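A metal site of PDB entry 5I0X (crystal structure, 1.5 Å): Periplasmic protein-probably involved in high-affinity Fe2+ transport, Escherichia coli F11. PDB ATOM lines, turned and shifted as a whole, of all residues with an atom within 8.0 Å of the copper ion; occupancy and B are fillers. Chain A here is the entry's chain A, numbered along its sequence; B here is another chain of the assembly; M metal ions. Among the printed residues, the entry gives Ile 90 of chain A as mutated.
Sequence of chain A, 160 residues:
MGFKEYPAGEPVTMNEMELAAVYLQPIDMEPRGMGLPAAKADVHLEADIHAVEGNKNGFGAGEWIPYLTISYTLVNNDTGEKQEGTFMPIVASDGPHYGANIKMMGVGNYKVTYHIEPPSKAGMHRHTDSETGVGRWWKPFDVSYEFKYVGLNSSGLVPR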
ATOM      1  N   VAL A  22      -7.958  21.840 -21.754  1.00  0.00           N
ATOM      2  CA  VAL A  22      -8.925  21.052 -20.993  1.00  0.00           C
ATOM      3  C   VAL A  22      -9.673  20.188 -21.972  1.00  0.00           C
ATOM      4  O   VAL A  22      -9.750  20.483 -23.155  1.00  0.00           O
ATOM      5  CB  VAL A  22      -9.967  21.922 -20.248  1.00  0.00           C
ATOM      6  CG1 VAL A  22      -9.343  22.698 -19.099  1.00  0.00           C
ATOM      7  CG2 VAL A  22     -10.706  22.834 -21.220  1.00  0.00           C
ATOM      8  N   LEU A  24     -13.424  17.593 -22.265  1.00  0.00           N
ATOM      9  CA  LEU A  24     -14.708  17.203 -21.686  1.00  0.00           C
ATOM     10  C   LEU A  24     -15.320  16.178 -22.602  1.00  0.00           C
ATOM     11  O   LEU A  24     -14.673  15.721 -23.549  1.00  0.00           O
ATOM     12  CB  LEU A  24     -15.603  18.417 -21.485  1.00  0.00           C
ATOM     13  CG  LEU A  24     -15.739  19.561 -22.466  1.00  0.00           C
ATOM     14  CD1 LEU A  24     -16.977  20.384 -22.147  1.00  0.00           C
ATOM     15  CD2 LEU A  24     -14.519  20.471 -22.382  1.00  0.00           C
ATOM     16  N   GLN A  25     -16.568  15.828 -22.319  1.00  0.00           N
ATOM     17  CA  GLN A  25     -17.374  14.952 -23.154  1.00  0.00           C
ATOM     18  C   GLN A  25     -17.531  15.536 -24.570  1.00  0.00           C
ATOM     19  O   GLN A  25     -17.530  16.770 -24.720  1.00  0.00           O
ATOM     20  CB  GLN A  25     -18.732  14.774 -22.479  1.00  0.00           C
ATOM     21  CG  GLN A  25     -19.306  16.067 -21.887  1.00  0.00           C
ATOM     22  CD  GLN A  25     -18.544  16.660 -20.694  1.00  0.00           C
ATOM     23  OE1 GLN A  25     -17.834  15.960 -19.957  1.00  0.00           O
ATOM     24  NE2 GLN A  25     -18.717  17.958 -20.483  1.00  0.00           N
ATOM     25  N   ILE A  27     -19.007  17.233 -27.766  1.00  0.00           N
ATOM     26  CA  ILE A  27     -20.075  18.223 -27.842  1.00  0.00           C
ATOM     27  C   ILE A  27     -20.509  18.410 -29.298  1.00  0.00           C
ATOM     28  O   ILE A  27     -19.688  18.633 -30.163  1.00  0.00           O
ATOM     29  CB  ILE A  27     -19.598  19.557 -27.213  1.00  0.00           C
ATOM     30  CG1 ILE A  27     -19.425  19.376 -25.706  1.00  0.00           C
ATOM     31  CG2 ILE A  27     -20.566  20.697 -27.541  1.00  0.00           C
ATOM     32  CD1 ILE A  27     -19.047  20.629 -24.956  1.00  0.00           C
ATOM     33  N   MET A  29     -21.691  20.452 -32.331  1.00  0.00           N
ATOM     34  CA  MET A  29     -21.495  21.851 -32.668  1.00  0.00           C
ATOM     35  C   MET A  29     -22.203  22.206 -33.958  1.00  0.00           C
ATOM     36  O   MET A  29     -22.443  21.326 -34.799  1.00  0.00           O
ATOM     37  CB  MET A  29     -20.013  22.186 -32.777  1.00  0.00           C
ATOM     38  CG  MET A  29     -19.282  22.139 -31.437  1.00  0.00           C
ATOM     39  SD  MET A  29     -17.547  22.644 -31.608  1.00  0.00           S
ATOM     40  CE  MET A  29     -16.939  21.103 -32.305  1.00  0.00           C
ATOM     41  N   HIS A  44     -14.013  16.202 -26.171  1.00  0.00           N
ATOM     42  CA  HIS A  44     -13.927  17.517 -26.791  1.00  0.00           C
ATOM     43  C   HIS A  44     -12.743  18.197 -26.172  1.00  0.00           C
ATOM     44  O   HIS A  44     -12.713  18.395 -24.983  1.00  0.00           O
ATOM     45  CB  HIS A  44     -15.231  18.261 -26.525  1.00  0.00           C
ATOM     46  CG  HIS A  44     -15.284  19.632 -27.144  1.00  0.00           C
ATOM     47  ND1 HIS A  44     -15.621  19.852 -28.437  1.00  0.00           N
ATOM     48  CD2 HIS A  44     -15.093  20.895 -26.578  1.00  0.00           C
ATOM     49  CE1 HIS A  44     -15.609  21.180 -28.681  1.00  0.00           C
ATOM     50  NE2 HIS A  44     -15.291  21.806 -27.551  1.00  0.00           N
ATOM     51  N   LEU A  45     -11.716  18.506 -26.981  1.00  0.00           N
ATOM     52  CA  LEU A  45     -10.459  19.109 -26.503  1.00  0.00           C
ATOM     53  C   LEU A  45     -10.428  20.611 -26.820  1.00  0.00           C
ATOM     54  O   LEU A  45     -10.761  21.021 -27.941  1.00  0.00           O
ATOM     55  CB  LEU A  45      -9.267  18.392 -27.140  1.00  0.00           C
ATOM     56  CG  LEU A  45      -7.883  18.828 -26.656  1.00  0.00           C
ATOM     57  CD1 LEU A  45      -7.662  18.578 -25.164  1.00  0.00           C
ATOM     58  CD2 LEU A  45      -6.797  18.149 -27.486  1.00  0.00           C
ATOM     59  N   GLU A  46     -10.050  21.388 -25.817  1.00  0.00           N
ATOM     60  CA  GLU A  46     -10.067  22.866 -25.861  1.00  0.00           C
ATOM     61  C   GLU A  46      -8.680  23.479 -25.678  1.00  0.00           C
ATOM     62  O   GLU A  46      -7.814  22.916 -24.982  1.00  0.00           O
ATOM     63  CB  GLU A  46     -10.948  23.420 -24.742  1.00  0.00           C
ATOM     64  CG  GLU A  46     -12.231  22.664 -24.481  1.00  0.00           C
ATOM     65  CD  GLU A  46     -13.408  23.208 -25.264  1.00  0.00           C
ATOM     66  OE1 GLU A  46     -13.297  23.343 -26.507  1.00  0.00           O
ATOM     67  OE2 GLU A  46     -14.462  23.496 -24.635  1.00  0.00           O
ATOM     68  N   ALA A  47      -8.497  24.647 -26.288  1.00  0.00           N
ATOM     69  CA  ALA A  47      -7.400  25.538 -25.950  1.00  0.00           C
ATOM     70  C   ALA A  47      -8.042  26.795 -25.383  1.00  0.00           C
ATOM     71  O   ALA A  47      -8.905  27.403 -26.031  1.00  0.00           O
ATOM     72  CB  ALA A  47      -6.586  25.898 -27.202  1.00  0.00           C
ATOM     73  N   MET A  88     -10.913  24.608 -34.202  1.00  0.00           N
ATOM     74  CA  MET A  88     -11.801  25.627 -34.741  1.00  0.00           C
ATOM     75  C   MET A  88     -12.056  26.695 -33.679  1.00  0.00           C
ATOM     76  O   MET A  88     -11.987  26.398 -32.475  1.00  0.00           O
ATOM     77  CB  MET A  88     -13.125  24.983 -35.138  1.00  0.00           C
ATOM     78  CG  MET A  88     -13.049  24.161 -36.404  1.00  0.00           C
ATOM     79  SD  MET A  88     -14.539  23.166 -36.507  1.00  0.00           S
ATOM     80  CE  MET A  88     -14.399  22.307 -34.943  1.00  0.00           C
ATOM     81  N   PRO A  89     -12.356  27.938 -34.094  1.00  0.00           N
ATOM     82  CA  PRO A  89     -12.867  28.921 -33.127  1.00  0.00           C
ATOM     83  C   PRO A  89     -14.302  28.540 -32.802  1.00  0.00           C
ATOM     84  O   PRO A  89     -15.057  28.145 -33.693  1.00  0.00           O
ATOM     85  CB  PRO A  89     -12.811  30.261 -33.879  1.00  0.00           C
ATOM     86  CG  PRO A  89     -12.430  29.942 -35.282  1.00  0.00           C
ATOM     87  CD  PRO A  89     -12.272  28.471 -35.462  1.00  0.00           C
ATOM     88  N   ILE A  90     -14.651  28.620 -31.518  1.00  0.00           N
ATOM     89  CA  ILE A  90     -15.946  28.107 -31.008  1.00  0.00           C
ATOM     90  C   ILE A  90     -16.446  29.057 -29.933  1.00  0.00           C
ATOM     91  O   ILE A  90     -15.669  29.560 -29.149  1.00  0.00           O
ATOM     92  CB  ILE A  90     -15.780  26.712 -30.366  1.00  0.00           C
ATOM     93  CG1 ILE A  90     -15.118  25.728 -31.335  1.00  0.00           C
ATOM     94  CG2 ILE A  90     -17.138  26.194 -29.924  1.00  0.00           C
ATOM     95  CD1 ILE A  90     -14.608  24.477 -30.649  1.00  0.00           C
ATOM     96  N   VAL A  91     -17.757  29.268 -29.882  1.00  0.00           N
ATOM     97  CA  VAL A  91     -18.327  29.984 -28.750  1.00  0.00           C
ATOM     98  C   VAL A  91     -19.221  29.064 -27.938  1.00  0.00           C
ATOM     99  O   VAL A  91     -19.968  28.265 -28.486  1.00  0.00           O
ATOM    100  CB  VAL A  91     -19.098  31.242 -29.172  1.00  0.00           C
ATOM    101  CG1 VAL A  91     -19.234  32.187 -27.992  1.00  0.00           C
ATOM    102  CG2 VAL A  91     -18.401  31.915 -30.342  1.00  0.00           C
ATOM    103  N   ALA A  92     -19.103  29.204 -26.627  1.00  0.00           N
ATOM    104  CA  ALA A  92     -19.944  28.490 -25.674  1.00  0.00           C
ATOM    105  C   ALA A  92     -20.517  29.525 -24.727  1.00  0.00           C
ATOM    106  O   ALA A  92     -20.230  30.725 -24.820  1.00  0.00           O
ATOM    107  CB  ALA A  92     -19.098  27.488 -24.919  1.00  0.00           C
ATOM    108  N   ASP A  94     -19.862  30.297 -21.774  1.00  0.00           N
ATOM    109  CA  ASP A  94     -18.894  31.068 -21.010  1.00  0.00           C
ATOM    110  C   ASP A  94     -17.827  31.705 -21.909  1.00  0.00           C
ATOM    111  O   ASP A  94     -16.781  32.140 -21.414  1.00  0.00           O
ATOM    112  CB  ASP A  94     -18.230  30.187 -19.973  1.00  0.00           C
ATOM    113  CG  ASP A  94     -17.263  29.232 -20.601  1.00  0.00           C
ATOM    114  OD1 ASP A  94     -17.566  28.772 -21.719  1.00  0.00           O
ATOM    115  OD2 ASP A  94     -16.185  28.982 -20.009  1.00  0.00           O
ATOM    116  N   GLY A  95     -18.075  31.764 -23.220  1.00  0.00           N
ATOM    117  CA  GLY A  95     -17.238  32.577 -24.070  1.00  0.00           C
ATOM    118  C   GLY A  95     -16.554  31.837 -25.206  1.00  0.00           C
ATOM    119  O   GLY A  95     -16.660  30.615 -25.348  1.00  0.00           O
ATOM    120  N   PRO A  96     -15.808  32.599 -26.005  1.00  0.00           N
ATOM    121  CA  PRO A  96     -15.064  32.050 -27.134  1.00  0.00           C
ATOM    122  C   PRO A  96     -13.837  31.241 -26.688  1.00  0.00           C
ATOM    123  O   PRO A  96     -13.199  31.537 -25.668  1.00  0.00           O
ATOM    124  CB  PRO A  96     -14.655  33.290 -27.899  1.00  0.00           C
ATOM    125  CG  PRO A  96     -14.508  34.350 -26.842  1.00  0.00           C
ATOM    126  CD  PRO A  96     -15.684  34.058 -25.931  1.00  0.00           C
ATOM    127  N   HIS A  97     -13.541  30.213 -27.464  1.00  0.00           N
ATOM    128  CA  HIS A  97     -12.346  29.390 -27.254  1.00  0.00           C
ATOM    129  C   HIS A  97     -12.000  28.725 -28.553  1.00  0.00           C
ATOM    130  O   HIS A  97     -12.565  29.078 -29.611  1.00  0.00           O
ATOM    131  CB  HIS A  97     -12.570  28.349 -26.147  1.00  0.00           C
ATOM    132  CG  HIS A  97     -13.689  27.359 -26.421  1.00  0.00           C
ATOM    133  ND1 HIS A  97     -14.980  27.649 -26.199  1.00  0.00           N
ATOM    134  CD2 HIS A  97     -13.654  26.053 -26.890  1.00  0.00           C
ATOM    135  CE1 HIS A  97     -15.743  26.579 -26.536  1.00  0.00           C
ATOM    136  NE2 HIS A  97     -14.923  25.594 -26.940  1.00  0.00           N
ATOM    137  N   TYR A  98     -11.023  27.807 -28.521  1.00  0.00           N
ATOM    138  CA  TYR A  98     -10.699  27.012 -29.704  1.00  0.00           C
ATOM    139  C   TYR A  98     -10.810  25.551 -29.294  1.00  0.00           C
ATOM    140  O   TYR A  98     -10.520  25.212 -28.136  1.00  0.00           O
ATOM    141  CB  TYR A  98      -9.258  27.272 -30.154  1.00  0.00           C
ATOM    142  CG  TYR A  98      -8.994  28.682 -30.551  1.00  0.00           C
ATOM    143  CD1 TYR A  98      -9.260  29.106 -31.851  1.00  0.00           C
ATOM    144  CD2 TYR A  98      -8.517  29.618 -29.615  1.00  0.00           C
ATOM    145  CE1 TYR A  98      -9.021  30.434 -32.227  1.00  0.00           C
ATOM    146  CE2 TYR A  98      -8.276  30.936 -29.976  1.00  0.00           C
ATOM    147  CZ  TYR A  98      -8.528  31.344 -31.282  1.00  0.00           C
ATOM    148  OH  TYR A  98      -8.279  32.656 -31.621  1.00  0.00           O
ATOM    149  N   GLY A  99     -11.174  24.675 -30.223  1.00  0.00           N
ATOM    150  CA  GLY A  99     -11.258  23.274 -29.870  1.00  0.00           C
ATOM    151  C   GLY A  99     -11.700  22.383 -30.995  1.00  0.00           C
ATOM    152  O   GLY A  99     -11.848  22.825 -32.131  1.00  0.00           O
ATOM    153  N   ALA A 100     -11.890  21.113 -30.653  1.00  0.00           N
ATOM    154  CA  ALA A 100     -12.368  20.101 -31.615  1.00  0.00           C
ATOM    155  C   ALA A 100     -12.838  18.882 -30.835  1.00  0.00           C
ATOM    156  O   ALA A 100     -12.290  18.556 -29.771  1.00  0.00           O
ATOM    157  CB  ALA A 100     -11.244  19.674 -32.549  1.00  0.00           C
ATOM    158  N   ASN A 101     -13.801  18.165 -31.408  1.00  0.00           N
ATOM    159  CA  ASN A 101     -14.068  16.799 -30.970  1.00  0.00           C
ATOM    160  C   ASN A 101     -12.961  15.877 -31.495  1.00  0.00           C
ATOM    161  O   ASN A 101     -12.538  15.988 -32.665  1.00  0.00           O
ATOM    162  CB  ASN A 101     -15.439  16.313 -31.488  1.00  0.00           C
ATOM    163  CG  ASN A 101     -16.609  17.058 -30.878  1.00  0.00           C
ATOM    164  OD1 ASN A 101     -17.606  17.330 -31.570  1.00  0.00           O
ATOM    165  ND2 ASN A 101     -16.521  17.376 -29.602  1.00  0.00           N
ATOM    166  N   HIS B 125     -17.691  28.291 -34.755  1.00  0.00           N
ATOM    167  CA  HIS B 125     -18.693  27.278 -34.409  1.00  0.00           C
ATOM    168  C   HIS B 125     -19.257  27.551 -33.054  1.00  0.00           C
ATOM    169  O   HIS B 125     -18.822  28.461 -32.355  1.00  0.00           O
ATOM    170  CB  HIS B 125     -18.051  25.899 -34.455  1.00  0.00           C
ATOM    171  CG  HIS B 125     -17.759  25.422 -35.840  1.00  0.00           C
ATOM    172  ND1 HIS B 125     -16.865  26.023 -36.652  1.00  0.00           N
ATOM    173  CD2 HIS B 125     -18.263  24.328 -36.554  1.00  0.00           C
ATOM    174  CE1 HIS B 125     -16.815  25.366 -37.832  1.00  0.00           C
ATOM    175  NE2 HIS B 125     -17.672  24.336 -37.773  1.00  0.00           N
ATOM    176  N   ARG B 126     -20.273  26.780 -32.659  1.00  0.00           N
ATOM    177  CA  ARG B 126     -20.885  26.961 -31.340  1.00  0.00           C
ATOM    178  C   ARG B 126     -21.228  25.621 -30.689  1.00  0.00           C
ATOM    179  O   ARG B 126     -21.718  24.714 -31.371  1.00  0.00           O
ATOM    180  CB  ARG B 126     -22.140  27.864 -31.407  1.00  0.00           C
ATOM    181  CG  ARG B 126     -23.261  27.403 -32.325  1.00  0.00           C
ATOM    182  CD  ARG B 126     -24.376  28.440 -32.392  1.00  0.00           C
ATOM    183  NE  ARG B 126     -25.281  28.037 -33.451  1.00  0.00           N
ATOM    184  CZ  ARG B 126     -26.347  27.270 -33.244  1.00  0.00           C
ATOM    185  NH1 ARG B 126     -27.119  26.906 -34.252  1.00  0.00           N
ATOM    186  NH2 ARG B 126     -26.657  26.895 -32.010  1.00  0.00           N
ATOM    187  N   HIS B 127     -21.013  25.529 -29.379  1.00  0.00           N
ATOM    188  CA  HIS B 127     -21.550  24.393 -28.598  1.00  0.00           C
ATOM    189  C   HIS B 127     -23.044  24.427 -28.684  1.00  0.00           C
ATOM    190  O   HIS B 127     -23.648  25.510 -28.663  1.00  0.00           O
ATOM    191  CB  HIS B 127     -21.160  24.499 -27.124  1.00  0.00           C
ATOM    192  CG  HIS B 127     -19.691  24.223 -26.843  1.00  0.00           C
ATOM    193  ND1 HIS B 127     -19.231  24.044 -25.584  1.00  0.00           N
ATOM    194  CD2 HIS B 127     -18.600  24.106 -27.694  1.00  0.00           C
ATOM    195  CE1 HIS B 127     -17.890  23.834 -25.633  1.00  0.00           C
ATOM    196  NE2 HIS B 127     -17.508  23.870 -26.931  1.00  0.00           N
ATOM    197  N   ASP B 129     -24.778  21.753 -26.715  1.00  0.00           N
ATOM    198  CA  ASP B 129     -25.220  20.978 -25.546  1.00  0.00           C
ATOM    199  C   ASP B 129     -26.047  21.830 -24.572  1.00  0.00           C
ATOM    200  O   ASP B 129     -25.965  23.046 -24.595  1.00  0.00           O
ATOM    201  CB  ASP B 129     -24.015  20.366 -24.816  1.00  0.00           C
ATOM    202  CG  ASP B 129     -23.135  21.430 -24.171  1.00  0.00           C
ATOM    203  OD1 ASP B 129     -22.480  22.184 -24.920  1.00  0.00           O
ATOM    204  OD2 ASP B 129     -23.100  21.495 -22.915  1.00  0.00           O
ATOM    205  N   THR B 132     -23.476  23.942 -21.846  1.00  0.00           N
ATOM    206  CA  THR B 132     -22.613  25.037 -22.332  1.00  0.00           C
ATOM    207  C   THR B 132     -23.003  25.628 -23.680  1.00  0.00           C
ATOM    208  O   THR B 132     -22.294  26.487 -24.215  1.00  0.00           O
ATOM    209  CB  THR B 132     -21.124  24.623 -22.393  1.00  0.00           C
ATOM    210  OG1 THR B 132     -20.938  23.660 -23.434  1.00  0.00           O
ATOM    211  CG2 THR B 132     -20.658  24.028 -21.052  1.00  0.00           C
HETATM  212 CU    CU M   1     -15.427  23.708 -27.174  1.00  0.00          CU
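A ring nitrogen (ND1) of His 44 sits at hydrogen-bond distance from the side-chain amide nitrogen (ND2) of Asn 101, 2.9 Å away. O of Val 22 sits at hydrogen-bond distance from N of Glu 46. The backbone carbonyl oxygen (O) of Ile 90 sits at hydrogen-bond distance from the backbone NH (N) of His 97 (2.8 Å). O of Leu 24 sits at hydrogen-bond distance from N of His 44 (2.7 Å). ND1 of His 127 of chain B lies within hydrogen-bond range of OG1 of Thr 132 of chain B, at 2.8 Å. O of Val 91 sits at hydrogen-bond distance from N of His 127 of chain B, at 3.1 Å.
Ile 90 touches the copper ion (CD1 to CU, 3.7 Å). Of the 27 residues printed, 5 come within 4 Å of the copper ion. The nearest printed residue that does not touch the copper ion is Gly 99 (5.0 Å).
The copper ion is bound by a ring nitrogen (NE2) of His 44 (1.9 Å), a ring nitrogen (NE2) of His 97 (2.0 Å), a ring nitrogen (NE2) of His 127 of chain B (2.1 Å) and the side-chain carboxylate (OE1) of Glu 46 (2.3 Å). Slightly farther from the copper ion lies the side-chain carboxylate (OE2) of Glu 46 (2.7 Å).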
